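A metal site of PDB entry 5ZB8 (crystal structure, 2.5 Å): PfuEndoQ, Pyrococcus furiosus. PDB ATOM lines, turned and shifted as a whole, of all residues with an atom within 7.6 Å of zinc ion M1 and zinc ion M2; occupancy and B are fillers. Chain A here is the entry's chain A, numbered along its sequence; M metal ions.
Zinc ion M2 is bound by a ring nitrogen (NE2) of His 10 (2.1 Å), the side-chain carboxylate of Glu 76 (2.2 Å), a ring nitrogen (NE2) of His 8 (2.2 Å) and the side-chain carboxylate of Asp 193 (2.4 Å).
Zinc ion M2 has four donor atoms within binding distance.
ND1 of His 84 binds zinc ion M1, 2.1 Å away.
The side-chain carboxylate (OE2) of Glu 76 binds zinc ion M1.
Zinc ion M1 is bound by NE2 of His 139, 2.2 Å away.
O of His 139 lies close to OG1 of Thr 142.
The side-chain carboxylate (OE1) of Glu 76 lies close to the guanidinium group (NH1) of Arg 114 (3.1 Å).
A ring nitrogen (ND1) of His 10 lies within hydrogen-bond range of the side-chain hydroxyl (OG) of Ser 14 (3.3 Å).
N of His 84 is in hydrogen-bond range of O of Thr 145 (3.1 Å).
O of His 84 sits at hydrogen-bond distance from N of Ala 138, at 3.0 Å.
O of Ala 194 lies within hydrogen-bond range of N of His 10 (3.2 Å).
The side-chain carboxylate (OE1) of Glu 78 is in hydrogen-bond range of a ring nitrogen (NE2) of His 84 (2.7 Å).
The side-chain carboxylate of Asp 42 sits at hydrogen-bond distance from a ring nitrogen (ND1) of His 10.
Arg 114 touches zinc ion M1 (NH1 to ZN, 3.6 Å).
Of the 26 residues printed, 5 come within 4 Å of zinc ion M1.
The nearest printed residue that does not touch zinc ion M1 is His 8 (4.2 Å).
Arg 114 touches zinc ion M2 (NH1 to ZN, 3.6 Å).
Within 4 Å of zinc ion M2: His 8, His 10, Glu 76, Arg 114 and Asp 193.
The nearest printed residue that does not touch zinc ion M2 is His 139 (4.6 Å).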
ATOM      1  N   HIS A   8      -6.045   3.897 -19.549  1.00  0.00           N
ATOM      2  CA  HIS A   8      -4.627   3.717 -19.240  1.00  0.00           C
ATOM      3  C   HIS A   8      -4.029   5.063 -18.891  1.00  0.00           C
ATOM      4  O   HIS A   8      -3.798   5.894 -19.766  1.00  0.00           O
ATOM      5  CB  HIS A   8      -3.885   3.063 -20.411  1.00  0.00           C
ATOM      6  CG  HIS A   8      -2.437   2.770 -20.131  1.00  0.00           C
ATOM      7  ND1 HIS A   8      -1.619   2.168 -21.058  1.00  0.00           N
ATOM      8  CD2 HIS A   8      -1.680   2.973 -19.029  1.00  0.00           C
ATOM      9  CE1 HIS A   8      -0.404   2.029 -20.542  1.00  0.00           C
ATOM     10  NE2 HIS A   8      -0.415   2.514 -19.316  1.00  0.00           N
ATOM     11  N   ILE A   9      -3.792   5.292 -17.593  1.00  0.00           N
ATOM     12  CA  ILE A   9      -3.087   6.455 -17.084  1.00  0.00           C
ATOM     13  C   ILE A   9      -2.134   5.990 -15.991  1.00  0.00           C
ATOM     14  O   ILE A   9      -2.036   4.794 -15.694  1.00  0.00           O
ATOM     15  CB  ILE A   9      -4.037   7.537 -16.543  1.00  0.00           C
ATOM     16  CG1 ILE A   9      -4.768   7.046 -15.295  1.00  0.00           C
ATOM     17  CG2 ILE A   9      -5.037   7.965 -17.610  1.00  0.00           C
ATOM     18  CD1 ILE A   9      -5.641   8.092 -14.640  1.00  0.00           C
ATOM     19  N   HIS A  10      -1.434   6.934 -15.380  1.00  0.00           N
ATOM     20  CA  HIS A  10      -0.512   6.632 -14.297  1.00  0.00           C
ATOM     21  C   HIS A  10      -0.679   7.657 -13.188  1.00  0.00           C
ATOM     22  O   HIS A  10      -1.012   8.819 -13.430  1.00  0.00           O
ATOM     23  CB  HIS A  10       0.947   6.593 -14.774  1.00  0.00           C
ATOM     24  CG  HIS A  10       1.265   5.398 -15.613  1.00  0.00           C
ATOM     25  ND1 HIS A  10       1.448   4.140 -15.081  1.00  0.00           N
ATOM     26  CD2 HIS A  10       1.432   5.266 -16.949  1.00  0.00           C
ATOM     27  CE1 HIS A  10       1.716   3.292 -16.049  1.00  0.00           C
ATOM     28  NE2 HIS A  10       1.707   3.946 -17.194  1.00  0.00           N
ATOM     29  N   SER A  14       4.051   6.617  -9.982  1.00  0.00           N
ATOM     30  CA  SER A  14       4.830   6.058 -11.075  1.00  0.00           C
ATOM     31  C   SER A  14       6.056   6.920 -11.373  1.00  0.00           C
ATOM     32  O   SER A  14       6.065   8.127 -11.107  1.00  0.00           O
ATOM     33  CB  SER A  14       3.987   5.914 -12.339  1.00  0.00           C
ATOM     34  OG  SER A  14       3.080   4.832 -12.245  1.00  0.00           O
ATOM     35  N   ASP A  42      -2.337   2.115 -11.980  1.00  0.00           N
ATOM     36  CA  ASP A  42      -1.509   1.819 -10.796  1.00  0.00           C
ATOM     37  C   ASP A  42      -2.297   1.129  -9.685  1.00  0.00           C
ATOM     38  O   ASP A  42      -1.999   1.306  -8.502  1.00  0.00           O
ATOM     39  CB  ASP A  42      -0.857   3.096 -10.262  1.00  0.00           C
ATOM     40  CG  ASP A  42       0.034   3.768 -11.278  1.00  0.00           C
ATOM     41  OD1 ASP A  42       0.052   3.337 -12.449  1.00  0.00           O
ATOM     42  OD2 ASP A  42       0.714   4.741 -10.904  1.00  0.00           O
ATOM     43  N   CYS A  75      -4.457  -1.226 -14.325  1.00  0.00           N
ATOM     44  CA  CYS A  75      -3.051  -1.192 -13.945  1.00  0.00           C
ATOM     45  C   CYS A  75      -2.219  -1.689 -15.120  1.00  0.00           C
ATOM     46  O   CYS A  75      -2.692  -2.434 -15.980  1.00  0.00           O
ATOM     47  CB  CYS A  75      -2.778  -2.036 -12.702  1.00  0.00           C
ATOM     48  SG  CYS A  75      -1.094  -1.876 -12.058  1.00  0.00           S
ATOM     49  N   GLU A  76      -0.954  -1.267 -15.147  1.00  0.00           N
ATOM     50  CA  GLU A  76       0.004  -1.666 -16.161  1.00  0.00           C
ATOM     51  C   GLU A  76       1.212  -2.294 -15.495  1.00  0.00           C
ATOM     52  O   GLU A  76       1.752  -1.737 -14.537  1.00  0.00           O
ATOM     53  CB  GLU A  76       0.437  -0.464 -17.019  1.00  0.00           C
ATOM     54  CG  GLU A  76       1.255  -0.842 -18.247  1.00  0.00           C
ATOM     55  CD  GLU A  76       1.948   0.356 -18.880  1.00  0.00           C
ATOM     56  OE1 GLU A  76       2.276   1.305 -18.149  1.00  0.00           O
ATOM     57  OE2 GLU A  76       2.166   0.344 -20.115  1.00  0.00           O
ATOM     58  N   VAL A  77       1.638  -3.455 -15.996  1.00  0.00           N
ATOM     59  CA  VAL A  77       2.773  -4.173 -15.438  1.00  0.00           C
ATOM     60  C   VAL A  77       3.829  -4.355 -16.522  1.00  0.00           C
ATOM     61  O   VAL A  77       3.545  -4.303 -17.718  1.00  0.00           O
ATOM     62  CB  VAL A  77       2.374  -5.537 -14.848  1.00  0.00           C
ATOM     63  CG1 VAL A  77       1.376  -5.354 -13.714  1.00  0.00           C
ATOM     64  CG2 VAL A  77       1.785  -6.433 -15.932  1.00  0.00           C
ATOM     65  N   GLU A  78       5.059  -4.584 -16.071  1.00  0.00           N
ATOM     66  CA  GLU A  78       6.208  -4.795 -16.942  1.00  0.00           C
ATOM     67  C   GLU A  78       6.785  -6.175 -16.652  1.00  0.00           C
ATOM     68  O   GLU A  78       7.025  -6.519 -15.494  1.00  0.00           O
ATOM     69  CB  GLU A  78       7.262  -3.699 -16.731  1.00  0.00           C
ATOM     70  CG  GLU A  78       8.562  -3.918 -17.464  1.00  0.00           C
ATOM     71  CD  GLU A  78       9.448  -2.686 -17.487  1.00  0.00           C
ATOM     72  OE1 GLU A  78       8.956  -1.612 -17.902  1.00  0.00           O
ATOM     73  OE2 GLU A  78      10.622  -2.786 -17.064  1.00  0.00           O
ATOM     74  N   ARG A  82      10.644  -6.543 -20.315  1.00  0.00           N
ATOM     75  CA  ARG A  82      10.262  -5.132 -20.264  1.00  0.00           C
ATOM     76  C   ARG A  82       9.035  -4.818 -21.132  1.00  0.00           C
ATOM     77  O   ARG A  82       8.811  -3.660 -21.482  1.00  0.00           O
ATOM     78  CB  ARG A  82      11.422  -4.213 -20.648  1.00  0.00           C
ATOM     79  CG  ARG A  82      12.398  -3.948 -19.506  1.00  0.00           C
ATOM     80  CD  ARG A  82      13.339  -2.797 -19.834  1.00  0.00           C
ATOM     81  NE  ARG A  82      13.683  -2.030 -18.641  1.00  0.00           N
ATOM     82  CZ  ARG A  82      13.057  -0.913 -18.277  1.00  0.00           C
ATOM     83  NH1 ARG A  82      12.063  -0.425 -19.018  1.00  0.00           N
ATOM     84  NH2 ARG A  82      13.429  -0.268 -17.171  1.00  0.00           N
ATOM     85  N   VAL A  83       8.243  -5.830 -21.469  1.00  0.00           N
ATOM     86  CA  VAL A  83       7.020  -5.617 -22.235  1.00  0.00           C
ATOM     87  C   VAL A  83       5.900  -5.196 -21.302  1.00  0.00           C
ATOM     88  O   VAL A  83       5.737  -5.757 -20.209  1.00  0.00           O
ATOM     89  CB  VAL A  83       6.648  -6.885 -23.025  1.00  0.00           C
ATOM     90  CG1 VAL A  83       5.290  -6.714 -23.710  1.00  0.00           C
ATOM     91  CG2 VAL A  83       7.712  -7.210 -24.050  1.00  0.00           C
ATOM     92  N   HIS A  84       5.129  -4.190 -21.709  1.00  0.00           N
ATOM     93  CA  HIS A  84       4.055  -3.651 -20.892  1.00  0.00           C
ATOM     94  C   HIS A  84       2.722  -4.294 -21.236  1.00  0.00           C
ATOM     95  O   HIS A  84       2.385  -4.480 -22.407  1.00  0.00           O
ATOM     96  CB  HIS A  84       3.962  -2.140 -21.077  1.00  0.00           C
ATOM     97  CG  HIS A  84       5.076  -1.373 -20.430  1.00  0.00           C
ATOM     98  ND1 HIS A  84       5.181  -0.001 -20.502  1.00  0.00           N
ATOM     99  CD2 HIS A  84       6.124  -1.791 -19.688  1.00  0.00           C
ATOM    100  CE1 HIS A  84       6.246   0.396 -19.839  1.00  0.00           C
ATOM    101  NE2 HIS A  84       6.848  -0.673 -19.335  1.00  0.00           N
ATOM    102  N   HIS A  85       1.967  -4.626 -20.190  1.00  0.00           N
ATOM    103  CA  HIS A  85       0.646  -5.242 -20.332  1.00  0.00           C
ATOM    104  C   HIS A  85      -0.356  -4.476 -19.495  1.00  0.00           C
ATOM    105  O   HIS A  85      -0.073  -4.096 -18.366  1.00  0.00           O
ATOM    106  CB  HIS A  85       0.674  -6.712 -19.901  1.00  0.00           C
ATOM    107  CG  HIS A  85       1.768  -7.516 -20.533  1.00  0.00           C
ATOM    108  ND1 HIS A  85       1.602  -8.209 -21.711  1.00  0.00           N
ATOM    109  CD2 HIS A  85       3.049  -7.743 -20.135  1.00  0.00           C
ATOM    110  CE1 HIS A  85       2.732  -8.830 -22.020  1.00  0.00           C
ATOM    111  NE2 HIS A  85       3.623  -8.563 -21.084  1.00  0.00           N
ATOM    112  N   LEU A  86      -1.538  -4.265 -20.064  1.00  0.00           N
ATOM    113  CA  LEU A  86      -2.617  -3.520 -19.410  1.00  0.00           C
ATOM    114  C   LEU A  86      -3.592  -4.504 -18.773  1.00  0.00           C
ATOM    115  O   LEU A  86      -3.994  -5.486 -19.404  1.00  0.00           O
ATOM    116  CB  LEU A  86      -3.336  -2.611 -20.401  1.00  0.00           C
ATOM    117  CG  LEU A  86      -4.520  -1.796 -19.905  1.00  0.00           C
ATOM    118  CD1 LEU A  86      -4.113  -0.863 -18.765  1.00  0.00           C
ATOM    119  CD2 LEU A  86      -5.144  -1.006 -21.043  1.00  0.00           C
ATOM    120  N   ARG A 114       4.168   1.382 -11.513  1.00  0.00           N
ATOM    121  CA  ARG A 114       4.135   0.319 -12.513  1.00  0.00           C
ATOM    122  C   ARG A 114       5.049  -0.815 -12.060  1.00  0.00           C
ATOM    123  O   ARG A 114       6.274  -0.733 -12.225  1.00  0.00           O
ATOM    124  CB  ARG A 114       4.592   0.849 -13.875  1.00  0.00           C
ATOM    125  CG  ARG A 114       4.631  -0.192 -14.983  1.00  0.00           C
ATOM    126  CD  ARG A 114       4.814   0.495 -16.331  1.00  0.00           C
ATOM    127  NE  ARG A 114       5.925   1.437 -16.301  1.00  0.00           N
ATOM    128  CZ  ARG A 114       6.001   2.527 -17.061  1.00  0.00           C
ATOM    129  NH1 ARG A 114       5.016   2.816 -17.900  1.00  0.00           N
ATOM    130  NH2 ARG A 114       7.042   3.334 -16.969  1.00  0.00           N
ATOM    131  N   ALA A 138      -0.072  -3.478 -23.836  1.00  0.00           N
ATOM    132  CA  ALA A 138      -0.173  -2.027 -23.864  1.00  0.00           C
ATOM    133  C   ALA A 138       0.661  -1.471 -25.017  1.00  0.00           C
ATOM    134  O   ALA A 138       1.720  -1.995 -25.343  1.00  0.00           O
ATOM    135  CB  ALA A 138       0.310  -1.426 -22.541  1.00  0.00           C
ATOM    136  N   HIS A 139       0.143  -0.388 -25.621  1.00  0.00           N
ATOM    137  CA  HIS A 139       0.758   0.312 -26.760  1.00  0.00           C
ATOM    138  C   HIS A 139       1.602  -0.621 -27.614  1.00  0.00           C
ATOM    139  O   HIS A 139       2.834  -0.480 -27.683  1.00  0.00           O
ATOM    140  CB  HIS A 139       1.606   1.493 -26.258  1.00  0.00           C
ATOM    141  CG  HIS A 139       2.395   1.193 -25.022  1.00  0.00           C
ATOM    142  ND1 HIS A 139       3.481   0.348 -25.015  1.00  0.00           N
ATOM    143  CD2 HIS A 139       2.247   1.627 -23.747  1.00  0.00           C
ATOM    144  CE1 HIS A 139       3.978   0.276 -23.790  1.00  0.00           C
ATOM    145  NE2 HIS A 139       3.246   1.041 -23.002  1.00  0.00           N
ATOM    146  N   THR A 142       4.477   0.617 -30.044  1.00  0.00           N
ATOM    147  CA  THR A 142       5.448   1.622 -29.626  1.00  0.00           C
ATOM    148  C   THR A 142       6.861   1.032 -29.691  1.00  0.00           C
ATOM    149  O   THR A 142       7.058  -0.147 -29.387  1.00  0.00           O
ATOM    150  CB  THR A 142       5.119   2.094 -28.205  1.00  0.00           C
ATOM    151  OG1 THR A 142       3.862   2.780 -28.215  1.00  0.00           O
ATOM    152  CG2 THR A 142       6.182   3.034 -27.653  1.00  0.00           C
ATOM    153  N   TRP A 144       9.267   0.916 -27.844  1.00  0.00           N
ATOM    154  CA  TRP A 144       9.916   0.578 -26.588  1.00  0.00           C
ATOM    155  C   TRP A 144       8.897   0.006 -25.622  1.00  0.00           C
ATOM    156  O   TRP A 144       7.725   0.419 -25.606  1.00  0.00           O
ATOM    157  CB  TRP A 144      10.605   1.799 -25.961  1.00  0.00           C
ATOM    158  CG  TRP A 144       9.754   3.027 -25.976  1.00  0.00           C
ATOM    159  CD1 TRP A 144       8.739   3.335 -25.119  1.00  0.00           C
ATOM    160  CD2 TRP A 144       9.846   4.115 -26.899  1.00  0.00           C
ATOM    161  NE1 TRP A 144       8.187   4.551 -25.452  1.00  0.00           N
ATOM    162  CE2 TRP A 144       8.853   5.050 -26.542  1.00  0.00           C
ATOM    163  CE3 TRP A 144      10.662   4.399 -27.995  1.00  0.00           C
ATOM    164  CZ2 TRP A 144       8.655   6.243 -27.241  1.00  0.00           C
ATOM    165  CZ3 TRP A 144      10.476   5.582 -28.687  1.00  0.00           C
ATOM    166  CH2 TRP A 144       9.483   6.486 -28.302  1.00  0.00           C
ATOM    167  N   THR A 145       9.349  -0.957 -24.814  1.00  0.00           N
ATOM    168  CA  THR A 145       8.533  -1.590 -23.766  1.00  0.00           C
ATOM    169  C   THR A 145       7.220  -2.103 -24.325  1.00  0.00           C
ATOM    170  O   THR A 145       6.166  -2.012 -23.691  1.00  0.00           O
ATOM    171  CB  THR A 145       8.278  -0.623 -22.605  1.00  0.00           C
ATOM    172  OG1 THR A 145       7.404   0.440 -23.028  1.00  0.00           O
ATOM    173  CG2 THR A 145       9.587  -0.016 -22.116  1.00  0.00           C
ATOM    174  N   SER A 146       7.269  -2.670 -25.530  1.00  0.00           N
ATOM    175  CA  SER A 146       6.056  -3.077 -26.229  1.00  0.00           C
ATOM    176  C   SER A 146       6.205  -4.474 -26.810  1.00  0.00           C
ATOM    177  O   SER A 146       7.310  -4.960 -27.048  1.00  0.00           O
ATOM    178  CB  SER A 146       5.708  -2.089 -27.340  1.00  0.00           C
ATOM    179  OG  SER A 146       5.419  -0.815 -26.803  1.00  0.00           O
ATOM    180  N   GLU A 167      -4.040  -2.776 -27.084  1.00  0.00           N
ATOM    181  CA  GLU A 167      -3.960  -1.322 -27.022  1.00  0.00           C
ATOM    182  C   GLU A 167      -3.070  -0.834 -28.153  1.00  0.00           C
ATOM    183  O   GLU A 167      -1.906  -1.252 -28.264  1.00  0.00           O
ATOM    184  CB  GLU A 167      -3.431  -0.859 -25.668  1.00  0.00           C
ATOM    185  CG  GLU A 167      -3.314   0.655 -25.542  1.00  0.00           C
ATOM    186  CD  GLU A 167      -2.872   1.091 -24.161  1.00  0.00           C
ATOM    187  OE1 GLU A 167      -3.722   1.158 -23.251  1.00  0.00           O
ATOM    188  OE2 GLU A 167      -1.666   1.369 -23.979  1.00  0.00           O
ATOM    189  N   SER A 192      -4.609   6.990 -23.514  1.00  0.00           N
ATOM    190  CA  SER A 192      -3.647   8.087 -23.586  1.00  0.00           C
ATOM    191  C   SER A 192      -2.298   7.730 -22.980  1.00  0.00           C
ATOM    192  O   SER A 192      -1.274   8.281 -23.414  1.00  0.00           O
ATOM    193  CB  SER A 192      -4.216   9.328 -22.888  1.00  0.00           C
ATOM    194  OG  SER A 192      -4.225   9.160 -21.482  1.00  0.00           O
ATOM    195  N   ASP A 193      -2.259   6.844 -21.992  1.00  0.00           N
ATOM    196  CA  ASP A 193      -1.059   6.593 -21.196  1.00  0.00           C
ATOM    197  C   ASP A 193      -0.575   7.901 -20.557  1.00  0.00           C
ATOM    198  O   ASP A 193       0.609   8.256 -20.625  1.00  0.00           O
ATOM    199  CB  ASP A 193       0.043   5.934 -22.034  1.00  0.00           C
ATOM    200  CG  ASP A 193       1.178   5.370 -21.195  1.00  0.00           C
ATOM    201  OD1 ASP A 193       1.042   5.332 -19.957  1.00  0.00           O
ATOM    202  OD2 ASP A 193       2.201   4.957 -21.775  1.00  0.00           O
ATOM    203  N   ALA A 194      -1.516   8.614 -19.951  1.00  0.00           N
ATOM    204  CA  ALA A 194      -1.264   9.977 -19.494  1.00  0.00           C
ATOM    205  C   ALA A 194      -0.291   9.997 -18.322  1.00  0.00           C
ATOM    206  O   ALA A 194      -0.457   9.252 -17.344  1.00  0.00           O
ATOM    207  CB  ALA A 194      -2.571  10.649 -19.104  1.00  0.00           C
ATOM    208  N   HIS A 195       0.724  10.843 -18.421  1.00  0.00           N
ATOM    209  CA  HIS A 195       1.660  11.091 -17.326  1.00  0.00           C
ATOM    210  C   HIS A 195       1.423  12.429 -16.642  1.00  0.00           C
ATOM    211  O   HIS A 195       2.159  12.777 -15.713  1.00  0.00           O
ATOM    212  CB  HIS A 195       3.101  11.005 -17.842  1.00  0.00           C
ATOM    213  CG  HIS A 195       3.557   9.619 -18.164  1.00  0.00           C
ATOM    214  ND1 HIS A 195       2.774   8.717 -18.860  1.00  0.00           N
ATOM    215  CD2 HIS A 195       4.711   8.970 -17.881  1.00  0.00           C
ATOM    216  CE1 HIS A 195       3.429   7.576 -18.984  1.00  0.00           C
ATOM    217  NE2 HIS A 195       4.608   7.704 -18.400  1.00  0.00           N
HETATM  218 ZN    ZN M   1       3.752   1.524 -20.965  1.00  0.00          ZN
HETATM  219 ZN    ZN M   2       1.724   3.198 -19.188  1.00  0.00          ZN
